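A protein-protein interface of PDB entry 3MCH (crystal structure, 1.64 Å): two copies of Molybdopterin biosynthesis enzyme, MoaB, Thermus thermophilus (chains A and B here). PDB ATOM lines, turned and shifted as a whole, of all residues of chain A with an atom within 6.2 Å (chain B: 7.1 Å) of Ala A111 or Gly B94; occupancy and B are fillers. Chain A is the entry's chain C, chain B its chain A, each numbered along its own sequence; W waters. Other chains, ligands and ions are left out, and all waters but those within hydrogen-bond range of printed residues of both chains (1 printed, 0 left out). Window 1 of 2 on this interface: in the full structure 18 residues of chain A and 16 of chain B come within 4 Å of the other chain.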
ATOM      1  N   MET A  99      34.233  20.281  -8.501  1.00  0.00           N
ATOM      2  CA  MET A  99      34.468  21.365  -9.446  1.00  0.00           C
ATOM      3  C   MET A  99      33.354  22.409  -9.424  1.00  0.00           C
ATOM      4  O   MET A  99      33.563  23.558  -9.824  1.00  0.00           O
ATOM      5  CB  MET A  99      34.659  20.809 -10.864  1.00  0.00           C
ATOM      6  CG  MET A  99      35.917  19.956 -11.003  1.00  0.00           C
ATOM      7  SD  MET A  99      36.333  19.520 -12.709  1.00  0.00           S
ATOM      8  CE  MET A  99      35.076  18.287 -13.063  1.00  0.00           C
ATOM      9  N   ARG A 100      32.169  22.023  -8.957  1.00  0.00           N
ATOM     10  CA  ARG A 100      31.057  22.970  -8.870  1.00  0.00           C
ATOM     11  C   ARG A 100      31.079  23.689  -7.524  1.00  0.00           C
ATOM     12  O   ARG A 100      30.182  24.472  -7.210  1.00  0.00           O
ATOM     13  CB  ARG A 100      29.710  22.260  -9.081  1.00  0.00           C
ATOM     14  CG  ARG A 100      29.384  21.999 -10.551  1.00  0.00           C
ATOM     15  CD  ARG A 100      27.930  21.574 -10.749  1.00  0.00           C
ATOM     16  NE  ARG A 100      27.705  20.164 -10.438  1.00  0.00           N
ATOM     17  CZ  ARG A 100      27.967  19.159 -11.270  1.00  0.00           C
ATOM     18  NH1 ARG A 100      28.465  19.402 -12.478  1.00  0.00           N
ATOM     19  NH2 ARG A 100      27.730  17.909 -10.896  1.00  0.00           N
ATOM     20  N   LEU A 101      32.121  23.418  -6.739  1.00  0.00           N
ATOM     21  CA  LEU A 101      32.305  24.044  -5.428  1.00  0.00           C
ATOM     22  C   LEU A 101      31.082  23.864  -4.543  1.00  0.00           C
ATOM     23  O   LEU A 101      30.688  24.777  -3.820  1.00  0.00           O
ATOM     24  CB  LEU A 101      32.592  25.538  -5.597  1.00  0.00           C
ATOM     25  CG  LEU A 101      33.683  25.936  -6.594  1.00  0.00           C
ATOM     26  CD1 LEU A 101      33.831  27.451  -6.611  1.00  0.00           C
ATOM     27  CD2 LEU A 101      34.995  25.270  -6.219  1.00  0.00           C
ATOM     28  N   VAL A 102      30.486  22.678  -4.594  1.00  0.00           N
ATOM     29  CA  VAL A 102      29.294  22.401  -3.807  1.00  0.00           C
ATOM     30  C   VAL A 102      29.531  22.504  -2.302  1.00  0.00           C
ATOM     31  O   VAL A 102      30.450  21.890  -1.762  1.00  0.00           O
ATOM     32  CB  VAL A 102      28.737  21.006  -4.136  1.00  0.00           C
ATOM     33  CG1 VAL A 102      27.456  20.763  -3.361  1.00  0.00           C
ATOM     34  CG2 VAL A 102      28.480  20.896  -5.632  1.00  0.00           C
ATOM     35  N   THR A 107      26.104  30.898  -2.787  1.00  0.00           N
ATOM     36  CA  THR A 107      25.832  30.192  -4.036  1.00  0.00           C
ATOM     37  C   THR A 107      26.838  30.636  -5.093  1.00  0.00           C
ATOM     38  O   THR A 107      26.911  31.816  -5.434  1.00  0.00           O
ATOM     39  CB  THR A 107      24.409  30.484  -4.538  1.00  0.00           C
ATOM     40  OG1 THR A 107      23.459  29.962  -3.598  1.00  0.00           O
ATOM     41  CG2 THR A 107      24.180  29.840  -5.905  1.00  0.00           C
ATOM     42  N   PRO A 108      27.633  29.691  -5.618  1.00  0.00           N
ATOM     43  CA  PRO A 108      28.639  30.009  -6.634  1.00  0.00           C
ATOM     44  C   PRO A 108      28.165  29.873  -8.075  1.00  0.00           C
ATOM     45  O   PRO A 108      27.294  29.058  -8.386  1.00  0.00           O
ATOM     46  CB  PRO A 108      29.751  29.026  -6.313  1.00  0.00           C
ATOM     47  CG  PRO A 108      28.967  27.790  -5.967  1.00  0.00           C
ATOM     48  CD  PRO A 108      27.831  28.323  -5.097  1.00  0.00           C
ATOM     49  N   MET A 109      28.752  30.676  -8.957  1.00  0.00           N
ATOM     50  CA  MET A 109      28.425  30.616 -10.372  1.00  0.00           C
ATOM     51  C   MET A 109      28.935  29.279 -10.903  1.00  0.00           C
ATOM     52  O   MET A 109      28.512  28.813 -11.960  1.00  0.00           O
ATOM     53  CB  MET A 109      29.108  31.757 -11.126  1.00  0.00           C
ATOM     54  CG  MET A 109      28.374  33.085 -11.081  1.00  0.00           C
ATOM     55  SD  MET A 109      26.819  33.046 -11.995  1.00  0.00           S
ATOM     56  CE  MET A 109      25.875  34.274 -11.083  1.00  0.00           C
ATOM     57  N   ALA A 110      29.857  28.672 -10.161  1.00  0.00           N
ATOM     58  CA  ALA A 110      30.432  27.384 -10.541  1.00  0.00           C
ATOM     59  C   ALA A 110      29.344  26.326 -10.672  1.00  0.00           C
ATOM     60  O   ALA A 110      29.501  25.345 -11.399  1.00  0.00           O
ATOM     61  CB  ALA A 110      31.464  26.943  -9.498  1.00  0.00           C
ATOM     62  N   ALA A 111      28.236  26.527  -9.967  1.00  0.00           N
ATOM     63  CA  ALA A 111      27.134  25.571 -10.010  1.00  0.00           C
ATOM     64  C   ALA A 111      26.534  25.445 -11.404  1.00  0.00           C
ATOM     65  O   ALA A 111      25.837  24.472 -11.700  1.00  0.00           O
ATOM     66  CB  ALA A 111      26.052  25.971  -9.005  1.00  0.00           C
ATOM     67  N   LEU A 112      26.808  26.421 -12.263  1.00  0.00           N
ATOM     68  CA  LEU A 112      26.275  26.389 -13.617  1.00  0.00           C
ATOM     69  C   LEU A 112      27.118  25.565 -14.582  1.00  0.00           C
ATOM     70  O   LEU A 112      26.753  25.407 -15.746  1.00  0.00           O
ATOM     71  CB  LEU A 112      26.100  27.811 -14.154  1.00  0.00           C
ATOM     72  CG  LEU A 112      25.074  28.669 -13.407  1.00  0.00           C
ATOM     73  CD1 LEU A 112      24.892  29.982 -14.148  1.00  0.00           C
ATOM     74  CD2 LEU A 112      23.745  27.934 -13.301  1.00  0.00           C
ATOM     75  N   SER A 113      28.243  25.036 -14.113  1.00  0.00           N
ATOM     76  CA  SER A 113      29.080  24.211 -14.980  1.00  0.00           C
ATOM     77  C   SER A 113      28.518  22.794 -15.043  1.00  0.00           C
ATOM     78  O   SER A 113      28.236  22.182 -14.012  1.00  0.00           O
ATOM     79  CB  SER A 113      30.520  24.152 -14.465  1.00  0.00           C
ATOM     80  OG  SER A 113      31.298  23.276 -15.271  1.00  0.00           O
ATOM     81  N   ARG A 114      28.358  22.278 -16.259  1.00  0.00           N
ATOM     82  CA  ARG A 114      27.839  20.935 -16.462  1.00  0.00           C
ATOM     83  C   ARG A 114      28.976  19.938 -16.670  1.00  0.00           C
ATOM     84  O   ARG A 114      28.750  18.806 -17.079  1.00  0.00           O
ATOM     85  CB  ARG A 114      26.908  20.910 -17.676  1.00  0.00           C
ATOM     86  CG  ARG A 114      25.665  21.767 -17.529  1.00  0.00           C
ATOM     87  CD  ARG A 114      24.878  21.800 -18.833  1.00  0.00           C
ATOM     88  NE  ARG A 114      25.710  22.332 -19.903  1.00  0.00           N
ATOM     89  CZ  ARG A 114      26.182  21.614 -20.918  1.00  0.00           C
ATOM     90  NH1 ARG A 114      25.894  20.322 -21.018  1.00  0.00           N
ATOM     91  NH2 ARG A 114      26.980  22.186 -21.811  1.00  0.00           N
ATOM     92  N   GLU B  91      20.643  18.330 -18.925  1.00  0.00           N
ATOM     93  CA  GLU B  91      20.459  18.617 -17.514  1.00  0.00           C
ATOM     94  C   GLU B  91      21.512  19.578 -16.990  1.00  0.00           C
ATOM     95  O   GLU B  91      22.594  19.713 -17.566  1.00  0.00           O
ATOM     96  CB  GLU B  91      20.502  17.327 -16.695  1.00  0.00           C
ATOM     97  CG  GLU B  91      19.249  16.483 -16.816  1.00  0.00           C
ATOM     98  CD  GLU B  91      19.292  15.255 -15.937  1.00  0.00           C
ATOM     99  OE1 GLU B  91      19.547  15.396 -14.722  1.00  0.00           O
ATOM    100  OE2 GLU B  91      19.067  14.146 -16.461  1.00  0.00           O
ATOM    101  N   VAL B  92      21.163  20.266 -15.909  1.00  0.00           N
ATOM    102  CA  VAL B  92      22.068  21.198 -15.242  1.00  0.00           C
ATOM    103  C   VAL B  92      22.113  20.681 -13.803  1.00  0.00           C
ATOM    104  O   VAL B  92      21.443  21.212 -12.917  1.00  0.00           O
ATOM    105  CB  VAL B  92      21.518  22.640 -15.270  1.00  0.00           C
ATOM    106  CG1 VAL B  92      22.523  23.592 -14.619  1.00  0.00           C
ATOM    107  CG2 VAL B  92      21.234  23.062 -16.705  1.00  0.00           C
ATOM    108  N   PRO B  93      22.903  19.621 -13.561  1.00  0.00           N
ATOM    109  CA  PRO B  93      23.043  19.001 -12.237  1.00  0.00           C
ATOM    110  C   PRO B  93      23.395  19.955 -11.098  1.00  0.00           C
ATOM    111  O   PRO B  93      22.956  19.761  -9.966  1.00  0.00           O
ATOM    112  CB  PRO B  93      24.113  17.934 -12.464  1.00  0.00           C
ATOM    113  CG  PRO B  93      24.932  18.509 -13.578  1.00  0.00           C
ATOM    114  CD  PRO B  93      23.890  19.064 -14.502  1.00  0.00           C
ATOM    115  N   GLY B  94      24.180  20.981 -11.401  1.00  0.00           N
ATOM    116  CA  GLY B  94      24.567  21.941 -10.381  1.00  0.00           C
ATOM    117  C   GLY B  94      23.383  22.626  -9.720  1.00  0.00           C
ATOM    118  O   GLY B  94      23.437  22.970  -8.535  1.00  0.00           O
ATOM    119  N   LEU B  95      22.307  22.829 -10.471  1.00  0.00           N
ATOM    120  CA  LEU B  95      21.127  23.482  -9.908  1.00  0.00           C
ATOM    121  C   LEU B  95      20.333  22.501  -9.054  1.00  0.00           C
ATOM    122  O   LEU B  95      19.709  22.890  -8.064  1.00  0.00           O
ATOM    123  CB  LEU B  95      20.249  24.053 -11.027  1.00  0.00           C
ATOM    124  CG  LEU B  95      20.849  25.259 -11.752  1.00  0.00           C
ATOM    125  CD1 LEU B  95      19.990  25.620 -12.961  1.00  0.00           C
ATOM    126  CD2 LEU B  95      20.941  26.444 -10.790  1.00  0.00           C
ATOM    127  N   ALA B  96      20.362  21.227  -9.437  1.00  0.00           N
ATOM    128  CA  ALA B  96      19.670  20.201  -8.678  1.00  0.00           C
ATOM    129  C   ALA B  96      20.379  20.067  -7.332  1.00  0.00           C
ATOM    130  O   ALA B  96      19.743  19.848  -6.310  1.00  0.00           O
ATOM    131  CB  ALA B  96      19.703  18.868  -9.435  1.00  0.00           C
ATOM    132  N   GLU B  97      21.701  20.204  -7.347  1.00  0.00           N
ATOM    133  CA  GLU B  97      22.497  20.110  -6.128  1.00  0.00           C
ATOM    134  C   GLU B  97      22.190  21.308  -5.227  1.00  0.00           C
ATOM    135  O   GLU B  97      22.005  21.160  -4.021  1.00  0.00           O
ATOM    136  CB  GLU B  97      23.990  20.070  -6.480  1.00  0.00           C
ATOM    137  CG  GLU B  97      24.412  18.783  -7.198  1.00  0.00           C
ATOM    138  CD  GLU B  97      25.742  18.905  -7.924  1.00  0.00           C
ATOM    139  OE1 GLU B  97      26.296  20.023  -7.998  1.00  0.00           O
ATOM    140  OE2 GLU B  97      26.228  17.875  -8.437  1.00  0.00           O
ATOM    141  N   LEU B  98      22.122  22.497  -5.813  1.00  0.00           N
ATOM    142  CA  LEU B  98      21.825  23.685  -5.013  1.00  0.00           C
ATOM    143  C   LEU B  98      20.475  23.559  -4.316  1.00  0.00           C
ATOM    144  O   LEU B  98      20.322  23.985  -3.171  1.00  0.00           O
ATOM    145  CB  LEU B  98      21.821  24.939  -5.886  1.00  0.00           C
ATOM    146  CG  LEU B  98      23.179  25.467  -6.345  1.00  0.00           C
ATOM    147  CD1 LEU B  98      22.958  26.662  -7.252  1.00  0.00           C
ATOM    148  CD2 LEU B  98      24.024  25.870  -5.133  1.00  0.00           C
ATOM    149  N   MET B  99      19.491  22.983  -5.007  1.00  0.00           N
ATOM    150  CA  MET B  99      18.156  22.820  -4.435  1.00  0.00           C
ATOM    151  C   MET B  99      18.122  21.809  -3.290  1.00  0.00           C
ATOM    152  O   MET B  99      17.186  21.806  -2.486  1.00  0.00           O
ATOM    153  CB  MET B  99      17.145  22.423  -5.517  1.00  0.00           C
ATOM    154  CG  MET B  99      16.942  23.488  -6.587  1.00  0.00           C
ATOM    155  SD  MET B  99      15.528  23.137  -7.677  1.00  0.00           S
ATOM    156  CE  MET B  99      16.204  21.816  -8.743  1.00  0.00           C
ATOM    157  N   ALA B 117      17.036  19.508 -12.839  1.00  0.00           N
ATOM    158  CA  ALA B 117      17.039  20.835 -13.448  1.00  0.00           C
ATOM    159  C   ALA B 117      17.590  20.642 -14.847  1.00  0.00           C
ATOM    160  O   ALA B 117      18.519  19.869 -15.047  1.00  0.00           O
ATOM    161  CB  ALA B 117      17.934  21.791 -12.656  1.00  0.00           C
ATOM    162  N   VAL B 142      19.144  28.777  -5.430  1.00  0.00           N
ATOM    163  CA  VAL B 142      19.494  29.002  -6.835  1.00  0.00           C
ATOM    164  C   VAL B 142      19.310  30.430  -7.339  1.00  0.00           C
ATOM    165  O   VAL B 142      19.885  30.804  -8.357  1.00  0.00           O
ATOM    166  CB  VAL B 142      18.685  28.070  -7.783  1.00  0.00           C
ATOM    167  CG1 VAL B 142      18.913  26.618  -7.407  1.00  0.00           C
ATOM    168  CG2 VAL B 142      17.213  28.417  -7.726  1.00  0.00           C
ATOM    169  N   VAL B 145      22.125  32.801  -9.025  1.00  0.00           N
ATOM    170  CA  VAL B 145      22.642  32.501 -10.361  1.00  0.00           C
ATOM    171  C   VAL B 145      21.545  32.299 -11.404  1.00  0.00           C
ATOM    172  O   VAL B 145      21.831  32.033 -12.569  1.00  0.00           O
ATOM    173  CB  VAL B 145      23.508  31.219 -10.351  1.00  0.00           C
ATOM    174  CG1 VAL B 145      24.622  31.345  -9.319  1.00  0.00           C
ATOM    175  CG2 VAL B 145      22.631  30.002 -10.056  1.00  0.00           C
HETATM  176  O   HOH W   1      25.443  22.264 -13.449  1.00  0.00           O
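The backbone carbonyl oxygen of Ser A113 sits at hydrogen-bond distance from the guanidinium group of Arg A100.
Of the 12 printed residues of chain A, 7 touch a printed residue of chain B.
Hydrophobic or aromatic side chains of chain A that line the printed part of chain B: Val A102, Met A109 and Ala A111.
Of the 12 printed residues of chain B, 6 touch a printed residue of chain A.
Hydrophobic or aromatic side chains of chain B that line the printed part of chain A: Pro B93, Leu B98 and Val B145.
Pro B93 touches Arg A100 (CG to NH1, 3.8 Å).
Gly B94 touches Arg A100 (CA to CD, 3.4 Å).
CG2 of Val A102 touches OE1 of Glu B97, at 3.3 Å.
Thr A107 touches Leu B98 (CG2 to CD1, 3.7 Å).
Thr A107 touches Val B145.
O of Pro A108 touches CG1 of Val B145, at 3.6 Å.
CG1 of Val B145 touches CE of Met A109 (3.6 Å).
Ala A111 touches Gly B94 (O to CA, 3.1 Å).
Leu B98 touches Ala A111.
Arg A114 touches Glu B91.
Water W1 lies within hydrogen-bond range of N of Gly B94 (2.7 Å), O of Ala A111 (2.8 Å) and O of Ser A113 (2.9 Å).
1 position is printed for both chains.
Of the 11 pairs that touch across the chains among the printed residues, none has its exchanged pair printed and touching as well.
OE1 of Glu B97 lies within salt-bridge range of NE of Arg A100 (2.8 Å).
Ala A111 touches two residues of chain B.
Of chain A, only Arg A100 (3.4 Å) and Ala A111 (3.1 Å) come within 4 Å of Gly B94.
Printed residues of chain B within 4 Å of Pro A108: Val B145 (3.6 Å).
Of the printed residues of chain B, Met A109 touches Val B145 (3.6 Å).
Ser A113 touches none of the printed residues of chain B.
The nearest residue of chain A that does not touch Gly B94 is Ser A113 (5.0 Å).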
